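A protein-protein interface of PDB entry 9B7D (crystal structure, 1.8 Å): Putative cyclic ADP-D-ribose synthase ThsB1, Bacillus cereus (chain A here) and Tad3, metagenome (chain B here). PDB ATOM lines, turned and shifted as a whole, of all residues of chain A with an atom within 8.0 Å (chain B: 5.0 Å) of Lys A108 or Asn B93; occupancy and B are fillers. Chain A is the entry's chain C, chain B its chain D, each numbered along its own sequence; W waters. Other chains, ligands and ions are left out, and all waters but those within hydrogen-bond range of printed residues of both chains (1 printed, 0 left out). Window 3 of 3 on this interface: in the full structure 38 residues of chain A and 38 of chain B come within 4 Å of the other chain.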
ATOM      1  N   ASP A  14       2.555  27.324  -2.058  1.00  0.00           N
ATOM      2  CA  ASP A  14       4.016  27.284  -2.107  1.00  0.00           C
ATOM      3  C   ASP A  14       4.601  26.748  -0.805  1.00  0.00           C
ATOM      4  O   ASP A  14       5.583  25.996  -0.822  1.00  0.00           O
ATOM      5  CB  ASP A  14       4.600  28.665  -2.424  1.00  0.00           C
ATOM      6  CG  ASP A  14       4.037  29.770  -1.545  1.00  0.00           C
ATOM      7  OD1 ASP A  14       3.451  29.472  -0.485  1.00  0.00           O
ATOM      8  OD2 ASP A  14       4.206  30.953  -1.914  1.00  0.00           O
ATOM      9  N   PHE A  18       6.942  22.642  -1.271  1.00  0.00           N
ATOM     10  CA  PHE A  18       8.321  22.223  -1.024  1.00  0.00           C
ATOM     11  C   PHE A  18       8.368  21.086  -0.015  1.00  0.00           C
ATOM     12  O   PHE A  18       9.225  20.199  -0.114  1.00  0.00           O
ATOM     13  CB  PHE A  18       9.192  23.413  -0.590  1.00  0.00           C
ATOM     14  CG  PHE A  18       9.146  23.745   0.883  1.00  0.00           C
ATOM     15  CD1 PHE A  18      10.019  23.142   1.781  1.00  0.00           C
ATOM     16  CD2 PHE A  18       8.291  24.733   1.353  1.00  0.00           C
ATOM     17  CE1 PHE A  18       9.994  23.472   3.129  1.00  0.00           C
ATOM     18  CE2 PHE A  18       8.269  25.072   2.696  1.00  0.00           C
ATOM     19  CZ  PHE A  18       9.121  24.440   3.585  1.00  0.00           C
ATOM     20  N   ARG A  19       7.436  21.077   0.932  1.00  0.00           N
ATOM     21  CA  ARG A  19       7.387  19.989   1.900  1.00  0.00           C
ATOM     22  C   ARG A  19       6.958  18.687   1.234  1.00  0.00           C
ATOM     23  O   ARG A  19       7.481  17.615   1.563  1.00  0.00           O
ATOM     24  CB  ARG A  19       6.462  20.383   3.051  1.00  0.00           C
ATOM     25  CG  ARG A  19       6.922  21.678   3.734  1.00  0.00           C
ATOM     26  CD  ARG A  19       6.118  22.042   4.986  1.00  0.00           C
ATOM     27  NE  ARG A  19       6.928  22.803   5.934  1.00  0.00           N
ATOM     28  CZ  ARG A  19       6.870  24.119   6.095  1.00  0.00           C
ATOM     29  NH1 ARG A  19       6.028  24.868   5.398  1.00  0.00           N
ATOM     30  NH2 ARG A  19       7.683  24.702   6.974  1.00  0.00           N
ATOM     31  N   PHE A 105       8.588  19.689   8.313  1.00  0.00           N
ATOM     32  CA  PHE A 105       9.780  19.960   7.518  1.00  0.00           C
ATOM     33  C   PHE A 105      10.134  21.437   7.633  1.00  0.00           C
ATOM     34  O   PHE A 105       9.273  22.305   7.462  1.00  0.00           O
ATOM     35  CB  PHE A 105       9.572  19.576   6.050  1.00  0.00           C
ATOM     36  CG  PHE A 105       9.419  18.092   5.819  1.00  0.00           C
ATOM     37  CD1 PHE A 105      10.426  17.215   6.195  1.00  0.00           C
ATOM     38  CD2 PHE A 105       8.297  17.583   5.184  1.00  0.00           C
ATOM     39  CE1 PHE A 105      10.296  15.854   5.987  1.00  0.00           C
ATOM     40  CE2 PHE A 105       8.164  16.221   4.963  1.00  0.00           C
ATOM     41  CZ  PHE A 105       9.164  15.355   5.368  1.00  0.00           C
ATOM     42  N   LYS A 106      11.399  21.721   7.931  1.00  0.00           N
ATOM     43  CA  LYS A 106      11.840  23.087   8.179  1.00  0.00           C
ATOM     44  C   LYS A 106      12.018  23.848   6.874  1.00  0.00           C
ATOM     45  O   LYS A 106      12.502  23.299   5.883  1.00  0.00           O
ATOM     46  CB  LYS A 106      13.159  23.091   8.951  1.00  0.00           C
ATOM     47  CG  LYS A 106      13.065  22.524  10.356  1.00  0.00           C
ATOM     48  CD  LYS A 106      14.436  22.430  11.010  1.00  0.00           C
ATOM     49  CE  LYS A 106      14.405  21.463  12.192  1.00  0.00           C
ATOM     50  NZ  LYS A 106      14.786  20.079  11.800  1.00  0.00           N
ATOM     51  N   ASP A 107      11.640  25.125   6.886  1.00  0.00           N
ATOM     52  CA  ASP A 107      11.884  25.999   5.746  1.00  0.00           C
ATOM     53  C   ASP A 107      13.314  26.538   5.837  1.00  0.00           C
ATOM     54  O   ASP A 107      14.115  26.109   6.673  1.00  0.00           O
ATOM     55  CB  ASP A 107      10.822  27.104   5.667  1.00  0.00           C
ATOM     56  CG  ASP A 107      10.912  28.133   6.810  1.00  0.00           C
ATOM     57  OD1 ASP A 107      11.940  28.231   7.510  1.00  0.00           O
ATOM     58  OD2 ASP A 107       9.921  28.862   7.013  1.00  0.00           O
ATOM     59  N   LYS A 108      13.647  27.509   4.984  1.00  0.00           N
ATOM     60  CA  LYS A 108      15.023  27.986   4.902  1.00  0.00           C
ATOM     61  C   LYS A 108      15.450  28.788   6.126  1.00  0.00           C
ATOM     62  O   LYS A 108      16.652  28.998   6.319  1.00  0.00           O
ATOM     63  CB  LYS A 108      15.202  28.824   3.636  1.00  0.00           C
ATOM     64  CG  LYS A 108      14.485  30.165   3.670  1.00  0.00           C
ATOM     65  CD  LYS A 108      14.829  30.998   2.439  1.00  0.00           C
ATOM     66  CE  LYS A 108      13.850  32.149   2.257  1.00  0.00           C
ATOM     67  NZ  LYS A 108      14.305  33.111   1.212  1.00  0.00           N
ATOM     68  N   TYR A 109      14.503  29.243   6.947  1.00  0.00           N
ATOM     69  CA  TYR A 109      14.820  29.911   8.204  1.00  0.00           C
ATOM     70  C   TYR A 109      14.818  28.956   9.390  1.00  0.00           C
ATOM     71  O   TYR A 109      15.106  29.384  10.510  1.00  0.00           O
ATOM     72  CB  TYR A 109      13.823  31.040   8.481  1.00  0.00           C
ATOM     73  CG  TYR A 109      13.731  32.087   7.397  1.00  0.00           C
ATOM     74  CD1 TYR A 109      14.663  33.109   7.308  1.00  0.00           C
ATOM     75  CD2 TYR A 109      12.700  32.055   6.469  1.00  0.00           C
ATOM     76  CE1 TYR A 109      14.572  34.073   6.312  1.00  0.00           C
ATOM     77  CE2 TYR A 109      12.601  33.007   5.475  1.00  0.00           C
ATOM     78  CZ  TYR A 109      13.536  34.011   5.401  1.00  0.00           C
ATOM     79  OH  TYR A 109      13.430  34.957   4.408  1.00  0.00           O
ATOM     80  N   GLY A 110      14.503  27.683   9.170  1.00  0.00           N
ATOM     81  CA  GLY A 110      14.374  26.729  10.252  1.00  0.00           C
ATOM     82  C   GLY A 110      12.993  26.639  10.862  1.00  0.00           C
ATOM     83  O   GLY A 110      12.822  25.926  11.857  1.00  0.00           O
ATOM     84  N   ASN A 111      12.004  27.331  10.301  1.00  0.00           N
ATOM     85  CA  ASN A 111      10.657  27.307  10.852  1.00  0.00           C
ATOM     86  C   ASN A 111       9.874  26.092  10.373  1.00  0.00           C
ATOM     87  O   ASN A 111      10.105  25.561   9.283  1.00  0.00           O
ATOM     88  CB  ASN A 111       9.888  28.570  10.469  1.00  0.00           C
ATOM     89  CG  ASN A 111      10.545  29.826  10.982  1.00  0.00           C
ATOM     90  OD1 ASN A 111      11.037  29.866  12.108  1.00  0.00           O
ATOM     91  ND2 ASN A 111      10.559  30.864  10.153  1.00  0.00           N
ATOM     92  N   GLU B  80      23.058  31.071  -1.056  1.00  0.00           N
ATOM     93  CA  GLU B  80      21.771  31.468  -0.494  1.00  0.00           C
ATOM     94  C   GLU B  80      20.581  30.780  -1.153  1.00  0.00           C
ATOM     95  O   GLU B  80      19.457  30.917  -0.658  1.00  0.00           O
ATOM     96  CB  GLU B  80      21.603  32.983  -0.603  1.00  0.00           C
ATOM     97  CG  GLU B  80      21.685  33.503  -2.028  1.00  0.00           C
ATOM     98  CD  GLU B  80      22.989  34.226  -2.307  1.00  0.00           C
ATOM     99  OE1 GLU B  80      22.938  35.356  -2.842  1.00  0.00           O
ATOM    100  OE2 GLU B  80      24.063  33.663  -1.991  1.00  0.00           O
ATOM    101  N   GLU B  81      20.784  30.058  -2.251  1.00  0.00           N
ATOM    102  CA  GLU B  81      19.671  29.435  -2.953  1.00  0.00           C
ATOM    103  C   GLU B  81      19.257  28.103  -2.352  1.00  0.00           C
ATOM    104  O   GLU B  81      18.360  27.455  -2.900  1.00  0.00           O
ATOM    105  CB  GLU B  81      20.020  29.227  -4.430  1.00  0.00           C
ATOM    106  CG  GLU B  81      18.871  29.520  -5.373  1.00  0.00           C
ATOM    107  CD  GLU B  81      19.264  29.386  -6.829  1.00  0.00           C
ATOM    108  OE1 GLU B  81      19.633  28.268  -7.255  1.00  0.00           O
ATOM    109  OE2 GLU B  81      19.234  30.414  -7.537  1.00  0.00           O
ATOM    110  N   TRP B  82      19.874  27.678  -1.251  1.00  0.00           N
ATOM    111  CA  TRP B  82      19.627  26.355  -0.697  1.00  0.00           C
ATOM    112  C   TRP B  82      19.117  26.450   0.734  1.00  0.00           C
ATOM    113  O   TRP B  82      19.439  27.387   1.470  1.00  0.00           O
ATOM    114  CB  TRP B  82      20.900  25.487  -0.740  1.00  0.00           C
ATOM    115  CG  TRP B  82      21.481  25.393  -2.119  1.00  0.00           C
ATOM    116  CD1 TRP B  82      22.444  26.193  -2.659  1.00  0.00           C
ATOM    117  CD2 TRP B  82      21.107  24.464  -3.150  1.00  0.00           C
ATOM    118  NE1 TRP B  82      22.703  25.815  -3.957  1.00  0.00           N
ATOM    119  CE2 TRP B  82      21.894  24.756  -4.281  1.00  0.00           C
ATOM    120  CE3 TRP B  82      20.187  23.408  -3.218  1.00  0.00           C
ATOM    121  CZ2 TRP B  82      21.794  24.033  -5.470  1.00  0.00           C
ATOM    122  CZ3 TRP B  82      20.088  22.687  -4.406  1.00  0.00           C
ATOM    123  CH2 TRP B  82      20.885  23.010  -5.516  1.00  0.00           C
ATOM    124  N   ASN B  83      18.311  25.459   1.114  1.00  0.00           N
ATOM    125  CA  ASN B  83      17.804  25.299   2.474  1.00  0.00           C
ATOM    126  C   ASN B  83      18.707  24.305   3.198  1.00  0.00           C
ATOM    127  O   ASN B  83      18.694  23.111   2.887  1.00  0.00           O
ATOM    128  CB  ASN B  83      16.354  24.814   2.436  1.00  0.00           C
ATOM    129  CG  ASN B  83      15.767  24.573   3.826  1.00  0.00           C
ATOM    130  OD1 ASN B  83      16.460  24.655   4.838  1.00  0.00           O
ATOM    131  ND2 ASN B  83      14.474  24.278   3.871  1.00  0.00           N
ATOM    132  N   ASN B  85      18.508  23.398   6.322  1.00  0.00           N
ATOM    133  CA  ASN B  85      17.864  22.841   7.514  1.00  0.00           C
ATOM    134  C   ASN B  85      17.393  21.407   7.261  1.00  0.00           C
ATOM    135  O   ASN B  85      16.220  21.062   7.391  1.00  0.00           O
ATOM    136  CB  ASN B  85      16.715  23.738   7.956  1.00  0.00           C
ATOM    137  CG  ASN B  85      17.200  25.063   8.482  1.00  0.00           C
ATOM    138  OD1 ASN B  85      17.920  25.114   9.479  1.00  0.00           O
ATOM    139  ND2 ASN B  85      16.846  26.145   7.794  1.00  0.00           N
ATOM    140  N   GLN B  91      17.649  21.227  -0.228  1.00  0.00           N
ATOM    141  CA  GLN B  91      16.611  21.547  -1.192  1.00  0.00           C
ATOM    142  C   GLN B  91      16.786  22.978  -1.690  1.00  0.00           C
ATOM    143  O   GLN B  91      17.134  23.876  -0.920  1.00  0.00           O
ATOM    144  CB  GLN B  91      15.243  21.370  -0.532  1.00  0.00           C
ATOM    145  CG  GLN B  91      14.043  21.640  -1.401  1.00  0.00           C
ATOM    146  CD  GLN B  91      12.763  21.256  -0.686  1.00  0.00           C
ATOM    147  OE1 GLN B  91      12.628  21.474   0.526  1.00  0.00           O
ATOM    148  NE2 GLN B  91      11.824  20.672  -1.419  1.00  0.00           N
ATOM    149  N   ASN B  92      16.568  23.181  -2.987  1.00  0.00           N
ATOM    150  CA  ASN B  92      16.681  24.519  -3.552  1.00  0.00           C
ATOM    151  C   ASN B  92      15.474  25.366  -3.155  1.00  0.00           C
ATOM    152  O   ASN B  92      14.334  24.890  -3.157  1.00  0.00           O
ATOM    153  CB  ASN B  92      16.802  24.442  -5.076  1.00  0.00           C
ATOM    154  CG  ASN B  92      17.257  25.748  -5.693  1.00  0.00           C
ATOM    155  OD1 ASN B  92      16.450  26.651  -5.905  1.00  0.00           O
ATOM    156  ND2 ASN B  92      18.557  25.855  -5.995  1.00  0.00           N
ATOM    157  N   ASN B  93      15.734  26.627  -2.792  1.00  0.00           N
ATOM    158  CA  ASN B  93      14.662  27.492  -2.306  1.00  0.00           C
ATOM    159  C   ASN B  93      13.769  27.993  -3.436  1.00  0.00           C
ATOM    160  O   ASN B  93      12.599  28.317  -3.201  1.00  0.00           O
ATOM    161  CB  ASN B  93      15.250  28.689  -1.565  1.00  0.00           C
ATOM    162  CG  ASN B  93      15.927  28.304  -0.283  1.00  0.00           C
ATOM    163  OD1 ASN B  93      15.470  27.407   0.437  1.00  0.00           O
ATOM    164  ND2 ASN B  93      17.029  28.982   0.021  1.00  0.00           N
ATOM    165  N   ARG B  94      14.303  28.088  -4.654  1.00  0.00           N
ATOM    166  CA  ARG B  94      13.573  28.694  -5.760  1.00  0.00           C
ATOM    167  C   ARG B  94      12.921  27.679  -6.686  1.00  0.00           C
ATOM    168  O   ARG B  94      11.985  28.036  -7.409  1.00  0.00           O
ATOM    169  CB  ARG B  94      14.506  29.598  -6.578  1.00  0.00           C
ATOM    170  CG  ARG B  94      14.933  30.854  -5.848  1.00  0.00           C
ATOM    171  CD  ARG B  94      15.982  31.595  -6.653  1.00  0.00           C
ATOM    172  NE  ARG B  94      15.382  32.195  -7.840  1.00  0.00           N
ATOM    173  CZ  ARG B  94      16.020  32.389  -8.984  1.00  0.00           C
ATOM    174  NH1 ARG B  94      17.292  32.055  -9.129  1.00  0.00           N
ATOM    175  NH2 ARG B  94      15.367  32.938 -10.007  1.00  0.00           N
ATOM    176  N   LEU B  95      13.397  26.435  -6.693  1.00  0.00           N
ATOM    177  CA  LEU B  95      12.801  25.349  -7.474  1.00  0.00           C
ATOM    178  C   LEU B  95      12.909  24.119  -6.573  1.00  0.00           C
ATOM    179  O   LEU B  95      13.931  23.422  -6.575  1.00  0.00           O
ATOM    180  CB  LEU B  95      13.507  25.158  -8.810  1.00  0.00           C
ATOM    181  CG  LEU B  95      12.926  24.110  -9.766  1.00  0.00           C
ATOM    182  CD1 LEU B  95      11.489  24.444 -10.118  1.00  0.00           C
ATOM    183  CD2 LEU B  95      13.781  23.977 -11.026  1.00  0.00           C
HETATM  184  O   HOH W   1      17.073  33.118   0.349  1.00  0.00           O
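The side-chain amide nitrogen (NE2) of Gln B91 is in hydrogen-bond range of the backbone carbonyl oxygen (O) of Phe A18 (2.9 Å).
ND2 of Asn B83 sits at hydrogen-bond distance from O of Lys A106.
The backbone carbonyl oxygen (O) of Asp A107 sits close to the side-chain amide oxygen (OD1) of Asn B83.
O of Asp A107 lies within hydrogen-bond range of ND2 of Asn B85 (3.0 Å).
The side-chain amide nitrogen (ND2) of Asn B85 is in hydrogen-bond range of the backbone carbonyl oxygen (O) of Lys A108, 3.2 Å away.
The backbone NH of Gly A110 sits close to the side-chain amide nitrogen of Asn B85 (3.1 Å).
Of the 10 printed residues of chain B, 4 touch a printed residue of chain A.
Hydrophobic or aromatic side chains of chain A that line the printed part of chain B: Phe A18.
Among the printed residues, 10 pairs touch across the chains.
Among the printed residues, no Asp or Glu carboxylate lies within 4 Å of a Lys or Arg side-chain nitrogen of the other chain.
Lys A108 touches just these residues of chain B: Asn B83, Asn B85 and Asn B93.
Asn B93 touches just one residue of chain A: Lys A108.
Of the printed residues of chain B, Lys A106 touches Asn B83 (3.0 Å) and Asn B85 (3.7 Å).
Of the printed residues of chain A, Gln B91 touches Phe A18 (2.9 Å).
Printed residues of chain A within 4 Å of Asn B85: Lys A106, Asp A107, Lys A108, Tyr A109 and Gly A110.
OD1 of Asp A107 sits at hydrogen-bond distance from N of Tyr A109 (2.8 Å).
N of Gly A110 lies within hydrogen-bond range of OD1 of Asp A107 (3.1 Å).
N of Asn A111 sits at hydrogen-bond distance from OD1 of Asp A107 (2.9 Å).
ND2 of Asn B93 sits at hydrogen-bond distance from O of Glu B80 (3.2 Å).
The backbone carbonyl oxygen (O) of Glu B81 lies within hydrogen-bond range of the backbone NH (N) of Asn B93 (2.8 Å).
The side-chain amide oxygen (OD1) of Asn B83 sits at hydrogen-bond distance from the backbone NH (N) of Asn B85, at 2.8 Å.
Among the printed residues, pairs that only touch across the chains: Lys A106 with Asn B85 (3.7 Å), Lys A108 with Asn B83 (3.5 Å), Lys A108 with Asn B93 (3.5 Å) and Tyr A109 with Asn B85 (3.8 Å).
Water W1 bridges NZ of Lys A108 (2.9 Å) and O of Glu B80 (3.4 Å).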
